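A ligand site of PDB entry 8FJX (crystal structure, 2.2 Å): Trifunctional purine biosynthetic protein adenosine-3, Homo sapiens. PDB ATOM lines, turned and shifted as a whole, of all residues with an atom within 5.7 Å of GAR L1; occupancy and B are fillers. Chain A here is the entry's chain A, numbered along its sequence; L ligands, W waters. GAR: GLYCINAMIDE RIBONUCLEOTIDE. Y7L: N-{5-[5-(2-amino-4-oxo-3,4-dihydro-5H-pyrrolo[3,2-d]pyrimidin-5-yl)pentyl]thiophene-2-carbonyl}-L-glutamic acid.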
ATOM      1  N   GLY A  10      20.532  15.162 -14.873  1.00  0.00           N
ATOM      2  CA  GLY A  10      20.060  16.036 -15.928  1.00  0.00           C
ATOM      3  C   GLY A  10      18.973  17.016 -15.534  1.00  0.00           C
ATOM      4  O   GLY A  10      19.108  17.748 -14.546  1.00  0.00           O
ATOM      5  N   THR A  11      17.882  17.021 -16.311  1.00  0.00           N
ATOM      6  CA  THR A  11      16.874  18.078 -16.205  1.00  0.00           C
ATOM      7  C   THR A  11      16.266  18.159 -14.807  1.00  0.00           C
ATOM      8  O   THR A  11      16.069  19.242 -14.262  1.00  0.00           O
ATOM      9  CB  THR A  11      15.782  17.843 -17.241  1.00  0.00           C
ATOM     10  OG1 THR A  11      16.379  17.665 -18.535  1.00  0.00           O
ATOM     11  CG2 THR A  11      14.808  19.014 -17.297  1.00  0.00           C
ATOM     12  N   GLY A  12      15.936  17.009 -14.212  1.00  0.00           N
ATOM     13  CA  GLY A  12      15.404  16.981 -12.869  1.00  0.00           C
ATOM     14  C   GLY A  12      13.924  17.224 -12.726  1.00  0.00           C
ATOM     15  O   GLY A  12      13.484  17.711 -11.682  1.00  0.00           O
ATOM     16  N   SER A  13      13.111  16.880 -13.736  1.00  0.00           N
ATOM     17  CA  SER A  13      11.669  17.025 -13.571  1.00  0.00           C
ATOM     18  C   SER A  13      11.145  16.086 -12.491  1.00  0.00           C
ATOM     19  O   SER A  13      10.247  16.459 -11.724  1.00  0.00           O
ATOM     20  CB  SER A  13      10.948  16.789 -14.901  1.00  0.00           C
ATOM     21  OG  SER A  13      11.104  15.452 -15.374  1.00  0.00           O
ATOM     22  N   ASN A  14      11.691  14.872 -12.402  1.00  0.00           N
ATOM     23  CA  ASN A  14      11.308  14.001 -11.294  1.00  0.00           C
ATOM     24  C   ASN A  14      11.749  14.590  -9.962  1.00  0.00           C
ATOM     25  O   ASN A  14      10.986  14.576  -8.982  1.00  0.00           O
ATOM     26  CB  ASN A  14      11.900  12.597 -11.478  1.00  0.00           C
ATOM     27  CG  ASN A  14      11.065  11.737 -12.398  1.00  0.00           C
ATOM     28  OD1 ASN A  14       9.984  11.292 -12.037  1.00  0.00           O
ATOM     29  ND2 ASN A  14      11.575  11.506 -13.596  1.00  0.00           N
ATOM     30  N   LEU A  15      12.963  15.119  -9.899  1.00  0.00           N
ATOM     31  CA  LEU A  15      13.389  15.841  -8.703  1.00  0.00           C
ATOM     32  C   LEU A  15      12.361  16.890  -8.316  1.00  0.00           C
ATOM     33  O   LEU A  15      11.921  16.957  -7.159  1.00  0.00           O
ATOM     34  CB  LEU A  15      14.757  16.483  -8.934  1.00  0.00           C
ATOM     35  CG  LEU A  15      15.140  17.516  -7.857  1.00  0.00           C
ATOM     36  CD1 LEU A  15      15.206  16.854  -6.494  1.00  0.00           C
ATOM     37  CD2 LEU A  15      16.453  18.209  -8.189  1.00  0.00           C
ATOM     38  N   ALA A  87      16.830   9.765  -9.513  1.00  0.00           N
ATOM     39  CA  ALA A  87      15.856  10.480 -10.354  1.00  0.00           C
ATOM     40  C   ALA A  87      16.589  10.992 -11.601  1.00  0.00           C
ATOM     41  O   ALA A  87      17.003  12.152 -11.662  1.00  0.00           O
ATOM     42  CB  ALA A  87      15.194  11.617  -9.576  1.00  0.00           C
ATOM     43  N   GLY A  88      16.719  10.125 -12.604  1.00  0.00           N
ATOM     44  CA  GLY A  88      17.510  10.452 -13.763  1.00  0.00           C
ATOM     45  C   GLY A  88      18.995  10.234 -13.571  1.00  0.00           C
ATOM     46  O   GLY A  88      19.799  10.816 -14.297  1.00  0.00           O
ATOM     47  N   PHE A  89      19.373   9.417 -12.586  1.00  0.00           N
ATOM     48  CA  PHE A  89      20.779   9.122 -12.327  1.00  0.00           C
ATOM     49  C   PHE A  89      21.272   8.093 -13.329  1.00  0.00           C
ATOM     50  O   PHE A  89      20.713   6.992 -13.422  1.00  0.00           O
ATOM     51  CB  PHE A  89      20.945   8.617 -10.897  1.00  0.00           C
ATOM     52  CG  PHE A  89      22.356   8.607 -10.416  1.00  0.00           C
ATOM     53  CD1 PHE A  89      23.038   9.807 -10.253  1.00  0.00           C
ATOM     54  CD2 PHE A  89      22.998   7.422 -10.135  1.00  0.00           C
ATOM     55  CE1 PHE A  89      24.341   9.815  -9.813  1.00  0.00           C
ATOM     56  CE2 PHE A  89      24.309   7.416  -9.688  1.00  0.00           C
ATOM     57  CZ  PHE A  89      24.981   8.617  -9.525  1.00  0.00           C
ATOM     58  N   MET A  90      22.339   8.438 -14.050  1.00  0.00           N
ATOM     59  CA  MET A  90      22.800   7.636 -15.177  1.00  0.00           C
ATOM     60  C   MET A  90      24.061   6.824 -14.875  1.00  0.00           C
ATOM     61  O   MET A  90      24.725   6.353 -15.800  1.00  0.00           O
ATOM     62  CB  MET A  90      23.046   8.540 -16.396  1.00  0.00           C
ATOM     63  CG  MET A  90      21.788   9.145 -16.999  1.00  0.00           C
ATOM     64  SD  MET A  90      20.478   7.924 -17.276  1.00  0.00           S
ATOM     65  CE  MET A  90      21.399   6.599 -18.065  1.00  0.00           C
ATOM     66  N   ASN A 107      14.331   3.939  -7.375  1.00  0.00           N
ATOM     67  CA  ASN A 107      14.673   4.392  -8.709  1.00  0.00           C
ATOM     68  C   ASN A 107      13.406   4.445  -9.561  1.00  0.00           C
ATOM     69  O   ASN A 107      12.534   3.576  -9.440  1.00  0.00           O
ATOM     70  CB  ASN A 107      15.696   3.478  -9.368  1.00  0.00           C
ATOM     71  CG  ASN A 107      15.933   3.819 -10.807  1.00  0.00           C
ATOM     72  OD1 ASN A 107      16.551   4.843 -11.106  1.00  0.00           O
ATOM     73  ND2 ASN A 107      15.415   3.000 -11.712  1.00  0.00           N
ATOM     74  N   ILE A 108      13.316   5.465 -10.404  1.00  0.00           N
ATOM     75  CA  ILE A 108      12.238   5.591 -11.383  1.00  0.00           C
ATOM     76  C   ILE A 108      12.772   5.143 -12.737  1.00  0.00           C
ATOM     77  O   ILE A 108      13.843   5.593 -13.170  1.00  0.00           O
ATOM     78  CB  ILE A 108      11.690   7.034 -11.426  1.00  0.00           C
ATOM     79  CG1 ILE A 108      10.573   7.168 -12.477  1.00  0.00           C
ATOM     80  CG2 ILE A 108      12.799   8.030 -11.696  1.00  0.00           C
ATOM     81  CD1 ILE A 108       9.294   6.423 -12.130  1.00  0.00           C
ATOM     82  N   HIS A 109      12.044   4.244 -13.392  1.00  0.00           N
ATOM     83  CA  HIS A 109      12.466   3.711 -14.673  1.00  0.00           C
ATOM     84  C   HIS A 109      11.323   3.874 -15.673  1.00  0.00           C
ATOM     85  O   HIS A 109      10.173   3.527 -15.356  1.00  0.00           O
ATOM     86  CB  HIS A 109      12.849   2.230 -14.553  1.00  0.00           C
ATOM     87  CG  HIS A 109      13.440   1.677 -15.803  1.00  0.00           C
ATOM     88  ND1 HIS A 109      14.739   1.932 -16.187  1.00  0.00           N
ATOM     89  CD2 HIS A 109      12.914   0.878 -16.765  1.00  0.00           C
ATOM     90  CE1 HIS A 109      14.990   1.312 -17.335  1.00  0.00           C
ATOM     91  NE2 HIS A 109      13.902   0.667 -17.696  1.00  0.00           N
ATOM     92  N   PRO A 110      11.600   4.375 -16.877  1.00  0.00           N
ATOM     93  CA  PRO A 110      10.542   4.731 -17.820  1.00  0.00           C
ATOM     94  C   PRO A 110      10.051   3.554 -18.654  1.00  0.00           C
ATOM     95  O   PRO A 110       9.945   3.644 -19.883  1.00  0.00           O
ATOM     96  CB  PRO A 110      11.212   5.795 -18.696  1.00  0.00           C
ATOM     97  CG  PRO A 110      12.644   5.313 -18.773  1.00  0.00           C
ATOM     98  CD  PRO A 110      12.935   4.598 -17.461  1.00  0.00           C
ATOM     99  N   GLY A 118      17.466  -1.199 -18.802  1.00  0.00           N
ATOM    100  CA  GLY A 118      18.570  -0.473 -19.374  1.00  0.00           C
ATOM    101  C   GLY A 118      18.217   0.933 -19.813  1.00  0.00           C
ATOM    102  O   GLY A 118      17.134   1.463 -19.570  1.00  0.00           O
ATOM    103  N   SER A 119      19.174   1.534 -20.527  1.00  0.00           N
ATOM    104  CA  SER A 119      19.262   2.989 -20.585  1.00  0.00           C
ATOM    105  C   SER A 119      18.327   3.623 -21.610  1.00  0.00           C
ATOM    106  O   SER A 119      17.990   4.804 -21.459  1.00  0.00           O
ATOM    107  CB  SER A 119      20.702   3.405 -20.868  1.00  0.00           C
ATOM    108  OG  SER A 119      21.229   2.652 -21.945  1.00  0.00           O
ATOM    109  N   HIS A 122      12.677   3.884 -23.818  1.00  0.00           N
ATOM    110  CA  HIS A 122      11.741   4.419 -24.803  1.00  0.00           C
ATOM    111  C   HIS A 122      12.100   3.949 -26.213  1.00  0.00           C
ATOM    112  O   HIS A 122      11.220   3.543 -26.982  1.00  0.00           O
ATOM    113  CB  HIS A 122      11.727   5.947 -24.756  1.00  0.00           C
ATOM    114  CG  HIS A 122      11.106   6.507 -23.515  1.00  0.00           C
ATOM    115  ND1 HIS A 122       9.861   6.114 -23.059  1.00  0.00           N
ATOM    116  CD2 HIS A 122      11.531   7.472 -22.660  1.00  0.00           C
ATOM    117  CE1 HIS A 122       9.566   6.787 -21.958  1.00  0.00           C
ATOM    118  NE2 HIS A 122      10.556   7.617 -21.697  1.00  0.00           N
ATOM    119  N   SER A 167       8.386   9.971 -24.080  1.00  0.00           N
ATOM    120  CA  SER A 167       8.974  10.278 -22.785  1.00  0.00           C
ATOM    121  C   SER A 167       8.264  11.446 -22.114  1.00  0.00           C
ATOM    122  O   SER A 167       8.209  11.526 -20.887  1.00  0.00           O
ATOM    123  CB  SER A 167      10.462  10.589 -22.933  1.00  0.00           C
ATOM    124  OG  SER A 167      10.636  11.784 -23.666  1.00  0.00           O
ATOM    125  N   VAL A 170       5.198   9.726 -20.618  1.00  0.00           N
ATOM    126  CA  VAL A 170       5.550   8.857 -19.503  1.00  0.00           C
ATOM    127  C   VAL A 170       5.959   9.683 -18.294  1.00  0.00           C
ATOM    128  O   VAL A 170       5.685   9.299 -17.155  1.00  0.00           O
ATOM    129  CB  VAL A 170       6.655   7.862 -19.922  1.00  0.00           C
ATOM    130  CG1 VAL A 170       7.161   7.099 -18.703  1.00  0.00           C
ATOM    131  CG2 VAL A 170       6.138   6.896 -20.960  1.00  0.00           C
ATOM    132  N   LYS A 171       6.622  10.822 -18.511  1.00  0.00           N
ATOM    133  CA  LYS A 171       7.106  11.601 -17.378  1.00  0.00           C
ATOM    134  C   LYS A 171       5.955  12.122 -16.518  1.00  0.00           C
ATOM    135  O   LYS A 171       6.116  12.242 -15.300  1.00  0.00           O
ATOM    136  CB  LYS A 171       7.963  12.774 -17.862  1.00  0.00           C
ATOM    137  CG  LYS A 171       9.468  12.484 -17.967  1.00  0.00           C
ATOM    138  CD  LYS A 171      10.198  13.760 -18.358  1.00  0.00           C
ATOM    139  CE  LYS A 171      11.534  13.511 -19.057  1.00  0.00           C
ATOM    140  NZ  LYS A 171      12.581  13.061 -18.114  1.00  0.00           N
ATOM    141  N   GLU A 174       5.525   9.358 -14.198  1.00  0.00           N
ATOM    142  CA  GLU A 174       6.612   9.311 -13.235  1.00  0.00           C
ATOM    143  C   GLU A 174       6.408  10.317 -12.114  1.00  0.00           C
ATOM    144  O   GLU A 174       6.587  10.011 -10.933  1.00  0.00           O
ATOM    145  CB  GLU A 174       7.938   9.554 -13.938  1.00  0.00           C
ATOM    146  CG  GLU A 174       8.253   8.550 -15.044  1.00  0.00           C
ATOM    147  CD  GLU A 174       9.504   8.921 -15.813  1.00  0.00           C
ATOM    148  OE1 GLU A 174      10.309   9.713 -15.276  1.00  0.00           O
ATOM    149  OE2 GLU A 174       9.682   8.444 -16.947  1.00  0.00           O
ATOM    150  N   HIS A 175       6.024  11.551 -12.475  1.00  0.00           N
ATOM    151  CA  HIS A 175       5.814  12.593 -11.491  1.00  0.00           C
ATOM    152  C   HIS A 175       4.662  12.286 -10.538  1.00  0.00           C
ATOM    153  O   HIS A 175       4.491  12.989  -9.539  1.00  0.00           O
ATOM    154  CB  HIS A 175       5.572  13.928 -12.203  1.00  0.00           C
ATOM    155  CG  HIS A 175       6.705  14.333 -13.092  1.00  0.00           C
ATOM    156  ND1 HIS A 175       6.555  15.275 -14.090  1.00  0.00           N
ATOM    157  CD2 HIS A 175       7.995  13.926 -13.149  1.00  0.00           C
ATOM    158  CE1 HIS A 175       7.709  15.431 -14.724  1.00  0.00           C
ATOM    159  NE2 HIS A 175       8.600  14.619 -14.161  1.00  0.00           N
HETATM  160  C1  GAR L   1      13.113  10.114 -16.548  1.00  0.00           C
HETATM  161  O6  GAR L   1      12.263  10.130 -17.692  1.00  0.00           O
HETATM  162  C2  GAR L   1      13.340   8.667 -16.095  1.00  0.00           C
HETATM  163  O8  GAR L   1      12.231   7.852 -16.419  1.00  0.00           O
HETATM  164  C3  GAR L   1      14.611   8.297 -16.880  1.00  0.00           C
HETATM  165  O4  GAR L   1      15.375   9.513 -16.983  1.00  0.00           O
HETATM  166  C5  GAR L   1      14.496  10.643 -16.954  1.00  0.00           C
HETATM  167  C10 GAR L   1      14.973  11.704 -15.991  1.00  0.00           C
HETATM  168  O12 GAR L   1      14.285  12.917 -16.275  1.00  0.00           O
HETATM  169  N19 GAR L   1      15.331   7.244 -16.235  1.00  0.00           N
HETATM  170  C21 GAR L   1      16.308   6.607 -16.877  1.00  0.00           C
HETATM  171  O22 GAR L   1      16.577   6.791 -18.051  1.00  0.00           O
HETATM  172  C23 GAR L   1      17.066   5.610 -16.033  1.00  0.00           C
HETATM  173  N24 GAR L   1      18.396   5.387 -16.554  1.00  0.00           N
HETATM  174  P15 GAR L   1      14.336  14.112 -15.208  1.00  0.00           P
HETATM  175  O16 GAR L   1      13.696  13.534 -13.958  1.00  0.00           O
HETATM  176  O17 GAR L   1      15.831  14.383 -15.084  1.00  0.00           O
HETATM  177  O18 GAR L   1      13.520  15.202 -15.865  1.00  0.00           O
HETATM  178  C8  Y7L L   2      20.855   0.662 -10.702  1.00  0.00           C
HETATM  179  N7  Y7L L   2      20.014   1.627 -11.138  1.00  0.00           N
HETATM  180  C5  Y7L L   2      21.986   2.578 -10.874  1.00  0.00           C
HETATM  181  C6  Y7L L   2      20.660   2.784 -11.244  1.00  0.00           C
HETATM  182  N1  Y7L L   2      23.078   0.365 -10.077  1.00  0.00           N
HETATM  183  C2  Y7L L   2      22.841  -0.920  -9.840  1.00  0.00           C
HETATM  184  N3  Y7L L   2      21.644  -1.470 -10.004  1.00  0.00           N
HETATM  185  C4  Y7L L   2      20.645  -0.725 -10.424  1.00  0.00           C
HETATM  186  C13 Y7L L   2      22.735   2.912 -16.929  1.00  0.00           C
HETATM  187  C14 Y7L L   2      22.189   3.594 -15.824  1.00  0.00           C
HETATM  188  C15 Y7L L   2      20.842   3.197 -15.510  1.00  0.00           C
HETATM  189  C16 Y7L L   2      20.324   2.209 -16.355  1.00  0.00           C
HETATM  190  C17 Y7L L   2      24.116   3.027 -17.557  1.00  0.00           C
HETATM  191  C20 Y7L L   2      26.401   3.999 -17.718  1.00  0.00           C
HETATM  192  C21 Y7L L   2      26.608   5.377 -18.347  1.00  0.00           C
HETATM  193  C22 Y7L L   2      25.825   5.452 -19.659  1.00  0.00           C
HETATM  194  C23 Y7L L   2      25.783   6.851 -20.290  1.00  0.00           C
HETATM  195  C26 Y7L L   2      27.483   3.659 -16.706  1.00  0.00           C
HETATM  196  C29 Y7L L   2      18.606   1.412 -11.430  1.00  0.00           C
HETATM  197  C30 Y7L L   2      18.227   2.147 -12.707  1.00  0.00           C
HETATM  198  C31 Y7L L   2      18.270   1.228 -13.931  1.00  0.00           C
HETATM  199  C32 Y7L L   2      18.062   2.047 -15.205  1.00  0.00           C
HETATM  200  C33 Y7L L   2      18.942   1.544 -16.333  1.00  0.00           C
HETATM  201  C9  Y7L L   2      22.101   1.200 -10.519  1.00  0.00           C
HETATM  202  N11 Y7L L   2      23.940  -1.747  -9.369  1.00  0.00           N
HETATM  203  N19 Y7L L   2      25.109   3.955 -17.052  1.00  0.00           N
HETATM  204  O10 Y7L L   2      19.367  -1.281 -10.604  1.00  0.00           O
HETATM  205  O18 Y7L L   2      24.380   2.338 -18.474  1.00  0.00           O
HETATM  206  O24 Y7L L   2      26.282   7.026 -21.585  1.00  0.00           O
HETATM  207  O25 Y7L L   2      25.243   7.922 -19.582  1.00  0.00           O
HETATM  208  O27 Y7L L   2      28.593   3.196 -17.095  1.00  0.00           O
HETATM  209  O28 Y7L L   2      27.247   3.825 -15.477  1.00  0.00           O
HETATM  210  S12 Y7L L   2      21.544   1.849 -17.465  1.00  0.00           S
HETATM  211  O   HOH W   1      14.956  14.109 -11.758  1.00  0.00           O
HETATM  212  O   HOH W   2      15.967   7.626 -13.109  1.00  0.00           O
HETATM  213  O   HOH W   3      18.176  13.820 -13.657  1.00  0.00           O
HETATM  214  O   HOH W   4      12.701   9.526 -20.305  1.00  0.00           O
HETATM  215  O   HOH W   5      17.098  14.285 -17.360  1.00  0.00           O
HETATM  216  O   HOH W   6       9.835   9.383 -19.772  1.00  0.00           O
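O18 of GAR L1 lies within hydrogen-bond range of N of Ser 13, at 2.7 Å.
The side-chain hydroxyl of Ser 13 sits at hydrogen-bond distance from an oxygen (O18) of GAR L1, at 2.5 Å.
The side-chain amino group of Lys 171 lies within salt-bridge range of an oxygen (O18) of GAR L1, 3.2 Å away.
OE2 of Glu 174 sits at hydrogen-bond distance from O8 of GAR L1.
The backbone NH of Gly 12 sits at hydrogen-bond distance from an oxygen (O17) of GAR L1, at 2.8 Å.
The backbone NH of Asn 14 lies within hydrogen-bond range of an oxygen (O16) of GAR L1, 2.9 Å away.
An oxygen (O16) of GAR L1 sits at hydrogen-bond distance from the side-chain amide nitrogen of Asn 14 (3.0 Å).
N24 of GAR L1 lies within hydrogen-bond range of SD of Met 90 (3.4 Å).
O of Met 90 is in hydrogen-bond range of N19 of Y7L L2 (2.7 Å).
OG of Ser 13 lies within hydrogen-bond range of NE2 of His 175 (2.9 Å).
ND1 of His 175 lies close to O of Lys 171, 3.3 Å away.
ND2 of Asn 14 lies within hydrogen-bond range of OE1 of Glu 174 (2.8 Å).
Water W1 lies within hydrogen-bond range of an oxygen (O16) of GAR L1, the backbone carbonyl oxygen (O) of Ala 87, the backbone NH (N) of Leu 15 and the backbone NH (N) of Asn 14.
Water W5 bridges O17 of GAR L1 (2.6 Å) and N of Thr 11 (3.0 Å).
Water W4 lies within hydrogen-bond range of an oxygen (O6) of GAR L1 (2.7 Å) and a ring nitrogen (NE2) of His 122 (3.2 Å).
Water W3 lies within hydrogen-bond range of O17 of GAR L1 (2.8 Å), O of Ala 87 (2.9 Å), N of Gly 10 (3.0 Å) and O of Gly 88 (3.5 Å).
Water W2 lies within hydrogen-bond range of the backbone NH (N) of Gly 88 (2.7 Å), the backbone carbonyl oxygen (O) of Ile 108 (2.9 Å), a nitrogen (N19) of GAR L1 (3.2 Å) and the side-chain amide oxygen (OD1) of Asn 107 (3.5 Å).
Water W6 lies within hydrogen-bond range of a ring nitrogen (NE2) of His 122, the backbone carbonyl oxygen of Ser 167, the side-chain carboxylate of Glu 174 and an oxygen (O6) of GAR L1.
Merely in contact with GAR L1: Pro 110 (3.2 Å), Thr 11 (3.6 Å), Gly 88 (3.6 Å) and Ile 108 (3.8 Å).
Along chain A the residues within 4 Å of GAR L1 span positions 11 to 174.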
